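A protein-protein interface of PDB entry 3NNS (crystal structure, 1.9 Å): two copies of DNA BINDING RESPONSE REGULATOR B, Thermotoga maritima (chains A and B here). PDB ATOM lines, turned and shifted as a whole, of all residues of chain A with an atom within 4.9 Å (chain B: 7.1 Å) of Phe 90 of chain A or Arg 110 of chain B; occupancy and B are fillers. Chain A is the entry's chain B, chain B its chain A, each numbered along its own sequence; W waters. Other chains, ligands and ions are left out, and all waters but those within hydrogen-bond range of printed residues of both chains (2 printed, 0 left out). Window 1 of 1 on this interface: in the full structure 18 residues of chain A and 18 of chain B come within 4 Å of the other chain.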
ATOM      1  N   VAL A  86     -23.658 -16.173  14.107  1.00  0.00           N
ATOM      2  CA  VAL A  86     -22.835 -15.769  12.969  1.00  0.00           C
ATOM      3  C   VAL A  86     -23.734 -15.124  11.917  1.00  0.00           C
ATOM      4  O   VAL A  86     -23.401 -14.073  11.371  1.00  0.00           O
ATOM      5  CB  VAL A  86     -22.087 -16.980  12.352  1.00  0.00           C
ATOM      6  CG1 VAL A  86     -21.370 -16.561  11.075  1.00  0.00           C
ATOM      7  CG2 VAL A  86     -21.083 -17.537  13.356  1.00  0.00           C
ATOM      8  N   LEU A  87     -24.884 -15.745  11.654  1.00  0.00           N
ATOM      9  CA  LEU A  87     -25.842 -15.232  10.673  1.00  0.00           C
ATOM     10  C   LEU A  87     -26.377 -13.859  11.066  1.00  0.00           C
ATOM     11  O   LEU A  87     -26.629 -13.014  10.205  1.00  0.00           O
ATOM     12  CB  LEU A  87     -27.007 -16.216  10.510  1.00  0.00           C
ATOM     13  CG  LEU A  87     -26.750 -17.414   9.587  1.00  0.00           C
ATOM     14  CD1 LEU A  87     -27.635 -18.578   9.988  1.00  0.00           C
ATOM     15  CD2 LEU A  87     -27.012 -17.003   8.143  1.00  0.00           C
ATOM     16  N   LYS A  88     -26.544 -13.633  12.367  1.00  0.00           N
ATOM     17  CA  LYS A  88     -27.040 -12.349  12.852  1.00  0.00           C
ATOM     18  C   LYS A  88     -25.994 -11.257  12.659  1.00  0.00           C
ATOM     19  O   LYS A  88     -26.326 -10.100  12.380  1.00  0.00           O
ATOM     20  CB  LYS A  88     -27.428 -12.443  14.336  1.00  0.00           C
ATOM     21  CG  LYS A  88     -28.761 -13.142  14.589  1.00  0.00           C
ATOM     22  CD  LYS A  88     -29.153 -13.111  16.071  1.00  0.00           C
ATOM     23  CE  LYS A  88     -29.251 -11.688  16.615  1.00  0.00           C
ATOM     24  NZ  LYS A  88     -30.232 -10.860  15.860  1.00  0.00           N
ATOM     25  N   GLY A  89     -24.728 -11.633  12.806  1.00  0.00           N
ATOM     26  CA  GLY A  89     -23.646 -10.680  12.635  1.00  0.00           C
ATOM     27  C   GLY A  89     -23.577 -10.141  11.222  1.00  0.00           C
ATOM     28  O   GLY A  89     -23.518  -8.927  11.021  1.00  0.00           O
ATOM     29  N   PHE A  90     -23.581 -11.040  10.240  1.00  0.00           N
ATOM     30  CA  PHE A  90     -23.525 -10.644   8.833  1.00  0.00           C
ATOM     31  C   PHE A  90     -24.812  -9.906   8.465  1.00  0.00           C
ATOM     32  O   PHE A  90     -24.805  -8.989   7.648  1.00  0.00           O
ATOM     33  CB  PHE A  90     -23.335 -11.880   7.939  1.00  0.00           C
ATOM     34  CG  PHE A  90     -21.920 -12.418   7.935  1.00  0.00           C
ATOM     35  CD1 PHE A  90     -20.881 -11.678   7.372  1.00  0.00           C
ATOM     36  CD2 PHE A  90     -21.624 -13.652   8.507  1.00  0.00           C
ATOM     37  CE1 PHE A  90     -19.573 -12.152   7.379  1.00  0.00           C
ATOM     38  CE2 PHE A  90     -20.306 -14.139   8.519  1.00  0.00           C
ATOM     39  CZ  PHE A  90     -19.282 -13.385   7.954  1.00  0.00           C
ATOM     40  N   GLU A  91     -25.910 -10.308   9.093  1.00  0.00           N
ATOM     41  CA  GLU A  91     -27.212  -9.698   8.864  1.00  0.00           C
ATOM     42  C   GLU A  91     -27.121  -8.230   9.267  1.00  0.00           C
ATOM     43  O   GLU A  91     -27.764  -7.364   8.672  1.00  0.00           O
ATOM     44  CB  GLU A  91     -28.263 -10.420   9.715  1.00  0.00           C
ATOM     45  CG  GLU A  91     -29.703 -10.107   9.378  1.00  0.00           C
ATOM     46  CD  GLU A  91     -30.673 -10.855  10.284  1.00  0.00           C
ATOM     47  OE1 GLU A  91     -30.722 -10.538  11.492  1.00  0.00           O
ATOM     48  OE2 GLU A  91     -31.377 -11.764   9.794  1.00  0.00           O
ATOM     49  N   ALA A  92     -26.295  -7.960  10.275  1.00  0.00           N
ATOM     50  CA  ALA A  92     -26.090  -6.607  10.786  1.00  0.00           C
ATOM     51  C   ALA A  92     -25.137  -5.795   9.912  1.00  0.00           C
ATOM     52  O   ALA A  92     -24.957  -4.593  10.129  1.00  0.00           O
ATOM     53  CB  ALA A  92     -25.546  -6.667  12.213  1.00  0.00           C
ATOM     54  N   GLY A  93     -24.506  -6.455   8.946  1.00  0.00           N
ATOM     55  CA  GLY A  93     -23.584  -5.767   8.057  1.00  0.00           C
ATOM     56  C   GLY A  93     -22.112  -6.020   8.334  1.00  0.00           C
ATOM     57  O   GLY A  93     -21.248  -5.330   7.789  1.00  0.00           O
ATOM     58  N   ALA A  94     -21.816  -7.010   9.170  1.00  0.00           N
ATOM     59  CA  ALA A  94     -20.432  -7.332   9.505  1.00  0.00           C
ATOM     60  C   ALA A  94     -19.692  -7.863   8.281  1.00  0.00           C
ATOM     61  O   ALA A  94     -20.266  -8.592   7.468  1.00  0.00           O
ATOM     62  CB  ALA A  94     -20.391  -8.364  10.628  1.00  0.00           C
ATOM     63  N   ASP A  95     -18.420  -7.504   8.150  1.00  0.00           N
ATOM     64  CA  ASP A  95     -17.627  -7.961   7.013  1.00  0.00           C
ATOM     65  C   ASP A  95     -16.897  -9.253   7.345  1.00  0.00           C
ATOM     66  O   ASP A  95     -16.339  -9.900   6.466  1.00  0.00           O
ATOM     67  CB  ASP A  95     -16.623  -6.887   6.583  1.00  0.00           C
ATOM     68  CG  ASP A  95     -17.300  -5.612   6.131  1.00  0.00           C
ATOM     69  OD1 ASP A  95     -17.386  -4.664   6.939  1.00  0.00           O
ATOM     70  OD2 ASP A  95     -17.763  -5.569   4.970  1.00  0.00           O
ATOM     71  N   ASP A  96     -16.902  -9.618   8.623  1.00  0.00           N
ATOM     72  CA  ASP A  96     -16.273 -10.845   9.075  1.00  0.00           C
ATOM     73  C   ASP A  96     -16.774 -11.165  10.476  1.00  0.00           C
ATOM     74  O   ASP A  96     -17.242 -10.283  11.197  1.00  0.00           O
ATOM     75  CB  ASP A  96     -14.753 -10.705   9.076  1.00  0.00           C
ATOM     76  CG  ASP A  96     -14.054 -11.972   8.621  1.00  0.00           C
ATOM     77  OD1 ASP A  96     -12.858 -11.888   8.288  1.00  0.00           O
ATOM     78  OD2 ASP A  96     -14.702 -13.052   8.599  1.00  0.00           O
ATOM     79  N   TYR A  97     -16.684 -12.439  10.847  1.00  0.00           N
ATOM     80  CA  TYR A  97     -17.137 -12.906  12.146  1.00  0.00           C
ATOM     81  C   TYR A  97     -16.095 -13.870  12.682  1.00  0.00           C
ATOM     82  O   TYR A  97     -15.950 -14.978  12.165  1.00  0.00           O
ATOM     83  CB  TYR A  97     -18.476 -13.628  12.000  1.00  0.00           C
ATOM     84  CG  TYR A  97     -19.213 -13.844  13.301  1.00  0.00           C
ATOM     85  CD1 TYR A  97     -20.236 -12.985  13.696  1.00  0.00           C
ATOM     86  CD2 TYR A  97     -18.887 -14.907  14.140  1.00  0.00           C
ATOM     87  CE1 TYR A  97     -20.922 -13.184  14.898  1.00  0.00           C
ATOM     88  CE2 TYR A  97     -19.562 -15.112  15.340  1.00  0.00           C
ATOM     89  CZ  TYR A  97     -20.575 -14.251  15.711  1.00  0.00           C
ATOM     90  OH  TYR A  97     -21.238 -14.466  16.899  1.00  0.00           O
ATOM     91  N   LEU B  25     -28.055 -15.375  -5.930  1.00  0.00           N
ATOM     92  CA  LEU B  25     -27.249 -14.153  -5.981  1.00  0.00           C
ATOM     93  C   LEU B  25     -26.886 -13.728  -7.405  1.00  0.00           C
ATOM     94  O   LEU B  25     -26.710 -12.539  -7.679  1.00  0.00           O
ATOM     95  CB  LEU B  25     -25.960 -14.332  -5.173  1.00  0.00           C
ATOM     96  CG  LEU B  25     -26.064 -14.639  -3.676  1.00  0.00           C
ATOM     97  CD1 LEU B  25     -24.664 -14.739  -3.088  1.00  0.00           C
ATOM     98  CD2 LEU B  25     -26.857 -13.543  -2.965  1.00  0.00           C
ATOM     99  N   VAL B  46     -16.678 -13.419  -7.594  1.00  0.00           N
ATOM    100  CA  VAL B  46     -16.272 -14.231  -6.458  1.00  0.00           C
ATOM    101  C   VAL B  46     -15.976 -15.638  -6.932  1.00  0.00           C
ATOM    102  O   VAL B  46     -16.664 -16.167  -7.804  1.00  0.00           O
ATOM    103  CB  VAL B  46     -17.378 -14.335  -5.394  1.00  0.00           C
ATOM    104  CG1 VAL B  46     -16.922 -15.249  -4.268  1.00  0.00           C
ATOM    105  CG2 VAL B  46     -17.728 -12.955  -4.860  1.00  0.00           C
ATOM    106  N   ILE B  75     -12.837 -17.066  -1.978  1.00  0.00           N
ATOM    107  CA  ILE B  75     -13.201 -17.697  -0.730  1.00  0.00           C
ATOM    108  C   ILE B  75     -12.756 -19.149  -0.806  1.00  0.00           C
ATOM    109  O   ILE B  75     -13.242 -19.907  -1.645  1.00  0.00           O
ATOM    110  CB  ILE B  75     -14.737 -17.651  -0.500  1.00  0.00           C
ATOM    111  CG1 ILE B  75     -15.230 -16.204  -0.545  1.00  0.00           C
ATOM    112  CG2 ILE B  75     -15.080 -18.290   0.846  1.00  0.00           C
ATOM    113  CD1 ILE B  75     -16.726 -16.038  -0.256  1.00  0.00           C
ATOM    114  N   ASP B  95      -9.404 -14.190   0.345  1.00  0.00           N
ATOM    115  CA  ASP B  95     -10.166 -13.117   0.967  1.00  0.00           C
ATOM    116  C   ASP B  95     -11.011 -13.665   2.099  1.00  0.00           C
ATOM    117  O   ASP B  95     -11.473 -12.924   2.962  1.00  0.00           O
ATOM    118  CB  ASP B  95     -11.029 -12.420  -0.075  1.00  0.00           C
ATOM    119  CG  ASP B  95     -10.196 -11.734  -1.140  1.00  0.00           C
ATOM    120  OD1 ASP B  95     -10.017 -12.316  -2.232  1.00  0.00           O
ATOM    121  OD2 ASP B  95      -9.705 -10.612  -0.865  1.00  0.00           O
ATOM    122  N   ASP B  96     -11.219 -14.975   2.082  1.00  0.00           N
ATOM    123  CA  ASP B  96     -11.967 -15.632   3.136  1.00  0.00           C
ATOM    124  C   ASP B  96     -11.560 -17.100   3.165  1.00  0.00           C
ATOM    125  O   ASP B  96     -11.019 -17.632   2.186  1.00  0.00           O
ATOM    126  CB  ASP B  96     -13.477 -15.479   2.923  1.00  0.00           C
ATOM    127  CG  ASP B  96     -14.247 -15.374   4.246  1.00  0.00           C
ATOM    128  OD1 ASP B  96     -15.470 -15.107   4.223  1.00  0.00           O
ATOM    129  OD2 ASP B  96     -13.619 -15.555   5.313  1.00  0.00           O
ATOM    130  N   TYR B  97     -11.789 -17.739   4.304  1.00  0.00           N
ATOM    131  CA  TYR B  97     -11.451 -19.138   4.485  1.00  0.00           C
ATOM    132  C   TYR B  97     -12.593 -19.806   5.233  1.00  0.00           C
ATOM    133  O   TYR B  97     -12.804 -19.539   6.415  1.00  0.00           O
ATOM    134  CB  TYR B  97     -10.171 -19.270   5.302  1.00  0.00           C
ATOM    135  CG  TYR B  97      -9.496 -20.616   5.178  1.00  0.00           C
ATOM    136  CD1 TYR B  97      -8.433 -20.798   4.299  1.00  0.00           C
ATOM    137  CD2 TYR B  97      -9.900 -21.699   5.955  1.00  0.00           C
ATOM    138  CE1 TYR B  97      -7.779 -22.027   4.202  1.00  0.00           C
ATOM    139  CE2 TYR B  97      -9.258 -22.931   5.863  1.00  0.00           C
ATOM    140  CZ  TYR B  97      -8.197 -23.085   4.987  1.00  0.00           C
ATOM    141  OH  TYR B  97      -7.536 -24.291   4.904  1.00  0.00           O
ATOM    142  N   VAL B  98     -13.327 -20.668   4.541  1.00  0.00           N
ATOM    143  CA  VAL B  98     -14.450 -21.375   5.141  1.00  0.00           C
ATOM    144  C   VAL B  98     -14.088 -22.855   5.210  1.00  0.00           C
ATOM    145  O   VAL B  98     -13.519 -23.412   4.271  1.00  0.00           O
ATOM    146  CB  VAL B  98     -15.729 -21.182   4.300  1.00  0.00           C
ATOM    147  CG1 VAL B  98     -16.890 -21.955   4.908  1.00  0.00           C
ATOM    148  CG2 VAL B  98     -16.060 -19.696   4.221  1.00  0.00           C
ATOM    149  N   PRO B 104     -24.422 -23.809   4.561  1.00  0.00           N
ATOM    150  CA  PRO B 104     -24.670 -23.099   3.301  1.00  0.00           C
ATOM    151  C   PRO B 104     -25.244 -21.693   3.464  1.00  0.00           C
ATOM    152  O   PRO B 104     -24.987 -20.811   2.644  1.00  0.00           O
ATOM    153  CB  PRO B 104     -25.614 -24.041   2.549  1.00  0.00           C
ATOM    154  CG  PRO B 104     -26.320 -24.778   3.657  1.00  0.00           C
ATOM    155  CD  PRO B 104     -25.191 -25.064   4.619  1.00  0.00           C
ATOM    156  N   GLU B 105     -26.012 -21.486   4.527  1.00  0.00           N
ATOM    157  CA  GLU B 105     -26.621 -20.189   4.777  1.00  0.00           C
ATOM    158  C   GLU B 105     -25.558 -19.158   5.164  1.00  0.00           C
ATOM    159  O   GLU B 105     -25.711 -17.965   4.899  1.00  0.00           O
ATOM    160  CB  GLU B 105     -27.664 -20.307   5.888  1.00  0.00           C
ATOM    161  CG  GLU B 105     -28.673 -19.183   5.868  1.00  0.00           C
ATOM    162  CD  GLU B 105     -29.567 -19.250   4.648  1.00  0.00           C
ATOM    163  OE1 GLU B 105     -30.093 -18.196   4.235  1.00  0.00           O
ATOM    164  OE2 GLU B 105     -29.749 -20.362   4.110  1.00  0.00           O
ATOM    165  N   ILE B 106     -24.479 -19.625   5.785  1.00  0.00           N
ATOM    166  CA  ILE B 106     -23.391 -18.744   6.189  1.00  0.00           C
ATOM    167  C   ILE B 106     -22.488 -18.429   4.998  1.00  0.00           C
ATOM    168  O   ILE B 106     -22.026 -17.299   4.840  1.00  0.00           O
ATOM    169  CB  ILE B 106     -22.564 -19.371   7.326  1.00  0.00           C
ATOM    170  CG1 ILE B 106     -23.406 -19.387   8.607  1.00  0.00           C
ATOM    171  CG2 ILE B 106     -21.273 -18.583   7.536  1.00  0.00           C
ATOM    172  CD1 ILE B 106     -22.768 -20.119   9.769  1.00  0.00           C
ATOM    173  N   LEU B 107     -22.246 -19.433   4.161  1.00  0.00           N
ATOM    174  CA  LEU B 107     -21.419 -19.237   2.973  1.00  0.00           C
ATOM    175  C   LEU B 107     -22.122 -18.223   2.075  1.00  0.00           C
ATOM    176  O   LEU B 107     -21.479 -17.381   1.448  1.00  0.00           O
ATOM    177  CB  LEU B 107     -21.227 -20.556   2.222  1.00  0.00           C
ATOM    178  CG  LEU B 107     -20.480 -20.433   0.888  1.00  0.00           C
ATOM    179  CD1 LEU B 107     -19.050 -19.967   1.136  1.00  0.00           C
ATOM    180  CD2 LEU B 107     -20.483 -21.767   0.167  1.00  0.00           C
ATOM    181  N   LEU B 108     -23.449 -18.307   2.023  1.00  0.00           N
ATOM    182  CA  LEU B 108     -24.235 -17.381   1.216  1.00  0.00           C
ATOM    183  C   LEU B 108     -23.979 -15.967   1.733  1.00  0.00           C
ATOM    184  O   LEU B 108     -23.665 -15.053   0.963  1.00  0.00           O
ATOM    185  CB  LEU B 108     -25.730 -17.711   1.325  1.00  0.00           C
ATOM    186  CG  LEU B 108     -26.702 -16.677   0.745  1.00  0.00           C
ATOM    187  CD1 LEU B 108     -26.610 -16.667  -0.777  1.00  0.00           C
ATOM    188  CD2 LEU B 108     -28.124 -17.008   1.187  1.00  0.00           C
ATOM    189  N   ALA B 109     -24.111 -15.795   3.046  1.00  0.00           N
ATOM    190  CA  ALA B 109     -23.885 -14.500   3.674  1.00  0.00           C
ATOM    191  C   ALA B 109     -22.465 -13.999   3.404  1.00  0.00           C
ATOM    192  O   ALA B 109     -22.264 -12.812   3.161  1.00  0.00           O
ATOM    193  CB  ALA B 109     -24.137 -14.597   5.176  1.00  0.00           C
ATOM    194  N   ARG B 110     -21.483 -14.900   3.439  1.00  0.00           N
ATOM    195  CA  ARG B 110     -20.097 -14.514   3.191  1.00  0.00           C
ATOM    196  C   ARG B 110     -19.895 -14.068   1.745  1.00  0.00           C
ATOM    197  O   ARG B 110     -19.159 -13.119   1.478  1.00  0.00           O
ATOM    198  CB  ARG B 110     -19.152 -15.670   3.521  1.00  0.00           C
ATOM    199  CG  ARG B 110     -19.000 -15.912   5.010  1.00  0.00           C
ATOM    200  CD  ARG B 110     -18.124 -17.115   5.311  1.00  0.00           C
ATOM    201  NE  ARG B 110     -17.847 -17.216   6.740  1.00  0.00           N
ATOM    202  CZ  ARG B 110     -17.061 -16.382   7.417  1.00  0.00           C
ATOM    203  NH1 ARG B 110     -16.455 -15.375   6.801  1.00  0.00           N
ATOM    204  NH2 ARG B 110     -16.893 -16.546   8.722  1.00  0.00           N
ATOM    205  N   VAL B 111     -20.555 -14.748   0.813  1.00  0.00           N
ATOM    206  CA  VAL B 111     -20.454 -14.384  -0.601  1.00  0.00           C
ATOM    207  C   VAL B 111     -21.138 -13.036  -0.836  1.00  0.00           C
ATOM    208  O   VAL B 111     -20.569 -12.132  -1.456  1.00  0.00           O
ATOM    209  CB  VAL B 111     -21.116 -15.455  -1.501  1.00  0.00           C
ATOM    210  CG1 VAL B 111     -21.129 -14.989  -2.952  1.00  0.00           C
ATOM    211  CG2 VAL B 111     -20.358 -16.771  -1.379  1.00  0.00           C
ATOM    212  N   LYS B 112     -22.356 -12.896  -0.320  1.00  0.00           N
ATOM    213  CA  LYS B 112     -23.121 -11.661  -0.486  1.00  0.00           C
ATOM    214  C   LYS B 112     -22.420 -10.409   0.029  1.00  0.00           C
ATOM    215  O   LYS B 112     -22.466  -9.360  -0.615  1.00  0.00           O
ATOM    216  CB  LYS B 112     -24.484 -11.777   0.203  1.00  0.00           C
ATOM    217  CG  LYS B 112     -25.272 -10.470   0.211  1.00  0.00           C
ATOM    218  CD  LYS B 112     -26.526 -10.531   1.080  1.00  0.00           C
ATOM    219  CE  LYS B 112     -27.607 -11.421   0.491  1.00  0.00           C
ATOM    220  NZ  LYS B 112     -27.226 -12.862   0.481  1.00  0.00           N
ATOM    221  N   ARG B 113     -21.777 -10.504   1.189  1.00  0.00           N
ATOM    222  CA  ARG B 113     -21.111  -9.339   1.751  1.00  0.00           C
ATOM    223  C   ARG B 113     -19.897  -8.878   0.954  1.00  0.00           C
ATOM    224  O   ARG B 113     -19.378  -7.786   1.179  1.00  0.00           O
ATOM    225  CB  ARG B 113     -20.763  -9.588   3.227  1.00  0.00           C
ATOM    226  CG  ARG B 113     -19.305  -9.491   3.608  1.00  0.00           C
ATOM    227  CD  ARG B 113     -18.587 -10.783   3.323  1.00  0.00           C
ATOM    228  NE  ARG B 113     -17.456 -10.981   4.221  1.00  0.00           N
ATOM    229  CZ  ARG B 113     -16.677 -12.054   4.204  1.00  0.00           C
ATOM    230  NH1 ARG B 113     -16.906 -13.024   3.330  1.00  0.00           N
ATOM    231  NH2 ARG B 113     -15.678 -12.164   5.064  1.00  0.00           N
ATOM    232  N   PHE B 114     -19.436  -9.711   0.025  1.00  0.00           N
ATOM    233  CA  PHE B 114     -18.317  -9.325  -0.829  1.00  0.00           C
ATOM    234  C   PHE B 114     -18.940  -8.711  -2.083  1.00  0.00           C
ATOM    235  O   PHE B 114     -18.451  -7.711  -2.610  1.00  0.00           O
ATOM    236  CB  PHE B 114     -17.456 -10.531  -1.217  1.00  0.00           C
ATOM    237  CG  PHE B 114     -16.453 -10.945  -0.164  1.00  0.00           C
ATOM    238  CD1 PHE B 114     -15.863 -10.001   0.674  1.00  0.00           C
ATOM    239  CD2 PHE B 114     -16.057 -12.275  -0.050  1.00  0.00           C
ATOM    240  CE1 PHE B 114     -14.892 -10.374   1.609  1.00  0.00           C
ATOM    241  CE2 PHE B 114     -15.085 -12.665   0.880  1.00  0.00           C
ATOM    242  CZ  PHE B 114     -14.501 -11.708   1.712  1.00  0.00           C
ATOM    243  N   LEU B 115     -20.039  -9.308  -2.540  1.00  0.00           N
ATOM    244  CA  LEU B 115     -20.742  -8.817  -3.724  1.00  0.00           C
ATOM    245  C   LEU B 115     -21.329  -7.427  -3.503  1.00  0.00           C
ATOM    246  O   LEU B 115     -21.568  -6.691  -4.458  1.00  0.00           O
ATOM    247  CB  LEU B 115     -21.860  -9.787  -4.126  1.00  0.00           C
ATOM    248  CG  LEU B 115     -21.423 -11.143  -4.672  1.00  0.00           C
ATOM    249  CD1 LEU B 115     -22.645 -11.994  -4.957  1.00  0.00           C
ATOM    250  CD2 LEU B 115     -20.601 -10.940  -5.935  1.00  0.00           C
ATOM    251  N   GLU B 116     -21.558  -7.070  -2.243  1.00  0.00           N
ATOM    252  CA  GLU B 116     -22.110  -5.762  -1.913  1.00  0.00           C
ATOM    253  C   GLU B 116     -21.031  -4.686  -1.966  1.00  0.00           C
ATOM    254  O   GLU B 116     -21.305  -3.503  -1.778  1.00  0.00           O
ATOM    255  CB  GLU B 116     -22.759  -5.803  -0.529  1.00  0.00           C
ATOM    256  CG  GLU B 116     -23.846  -6.857  -0.427  1.00  0.00           C
ATOM    257  CD  GLU B 116     -24.520  -6.885   0.925  1.00  0.00           C
ATOM    258  OE1 GLU B 116     -23.805  -6.921   1.948  1.00  0.00           O
ATOM    259  OE2 GLU B 116     -25.769  -6.884   0.962  1.00  0.00           O
HETATM  260  O   HOH W   1     -19.390  -5.611   2.578  1.00  0.00           O
HETATM  261  O   HOH W   2     -14.165 -16.115  10.221  1.00  0.00           O
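The side-chain carboxylate of Asp 96 of chain B is in salt-bridge range of the guanidinium group of Arg 110 of chain B, 2.8 Å away. OD1 of Asp 96 of chain B is in salt-bridge range of NH1 of Arg 113 of chain B (2.7 Å). The guanidinium group (NH1) of Arg 113 of chain B sits at hydrogen-bond distance from the backbone carbonyl oxygen (O) of Arg 110 of chain B, at 2.9 Å.
Of the 12 printed residues of chain A, 5 touch a printed residue of chain B. Hydrophobic or aromatic side chains of chain A that line the printed part of chain B: Leu 87 and Phe 90. Of the 20 printed residues of chain B, 4 touch a printed residue of chain A. Printed residues of chain B that touch a printed residue of chain A: Glu 105, Ala 109, Arg 110 and Arg 113. Hydrophobic or aromatic side chains of chain B that line the printed part of chain A: Ala 109.
Phe 90 of chain A touches three residues of chain B. No residue of chain B comes within 4 Å of Gly 89 of chain A. Printed residues of chain B within 4 Å of Asp 95 of chain A: Arg 113. Printed residues of chain A within 4 Å of Ala 109 of chain B: Phe 90 (3.96 Å). Printed residues of chain A within 4 Å of Glu 105 of chain B: Leu 87. Of the printed residues of chain B, Asp 96 of chain A touches Arg 110 and Arg 113. The nearest residue of chain B that does not touch Phe 90 of chain A is Ile 106 of chain B (4.7 Å). The nearest printed residue of chain A that does not touch Arg 110 of chain B is Val 86 of chain A (5.1 Å). The nearest printed residue of chain B that does not touch Tyr 97 of chain A is Arg 113 of chain B (5.9 Å).
Positions printed for both chains: 95, 96 and 97. Of the 8 pairs that touch across the chains among the printed residues, none has its exchanged pair printed and touching as well.
NH2 of Arg 113 of chain B is in salt-bridge range of OD2 of Asp 96 of chain A. The guanidinium group of Arg 113 of chain B sits at hydrogen-bond distance from the backbone carbonyl oxygen of Asp 95 of chain A (2.7 Å). NH1 of Arg 110 of chain B is in salt-bridge range of OD2 of Asp 96 of chain A (3.4 Å).
Among the printed residues, merely in contact across the chains: Leu 87 of chain A with Glu 105 of chain B (3.6 Å), Phe 90 of chain A with Arg 110 of chain B (3.6 Å), Tyr 97 of chain A with Arg 110 of chain B (3.9 Å), Phe 90 of chain A with Ala 109 of chain B (3.96 Å) and Phe 90 of chain A with Arg 113 of chain B (3.98 Å).
Water W1 lies within hydrogen-bond range of the backbone carbonyl oxygen (O) of Arg 113 of chain B (2.6 Å) and the side-chain carboxylate (OD2) of Asp 95 of chain A (2.9 Å). Water W2 lies within hydrogen-bond range of the backbone carbonyl oxygen (O) of Tyr 97 of chain A and the guanidinium group (NH2) of Arg 110 of chain B.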
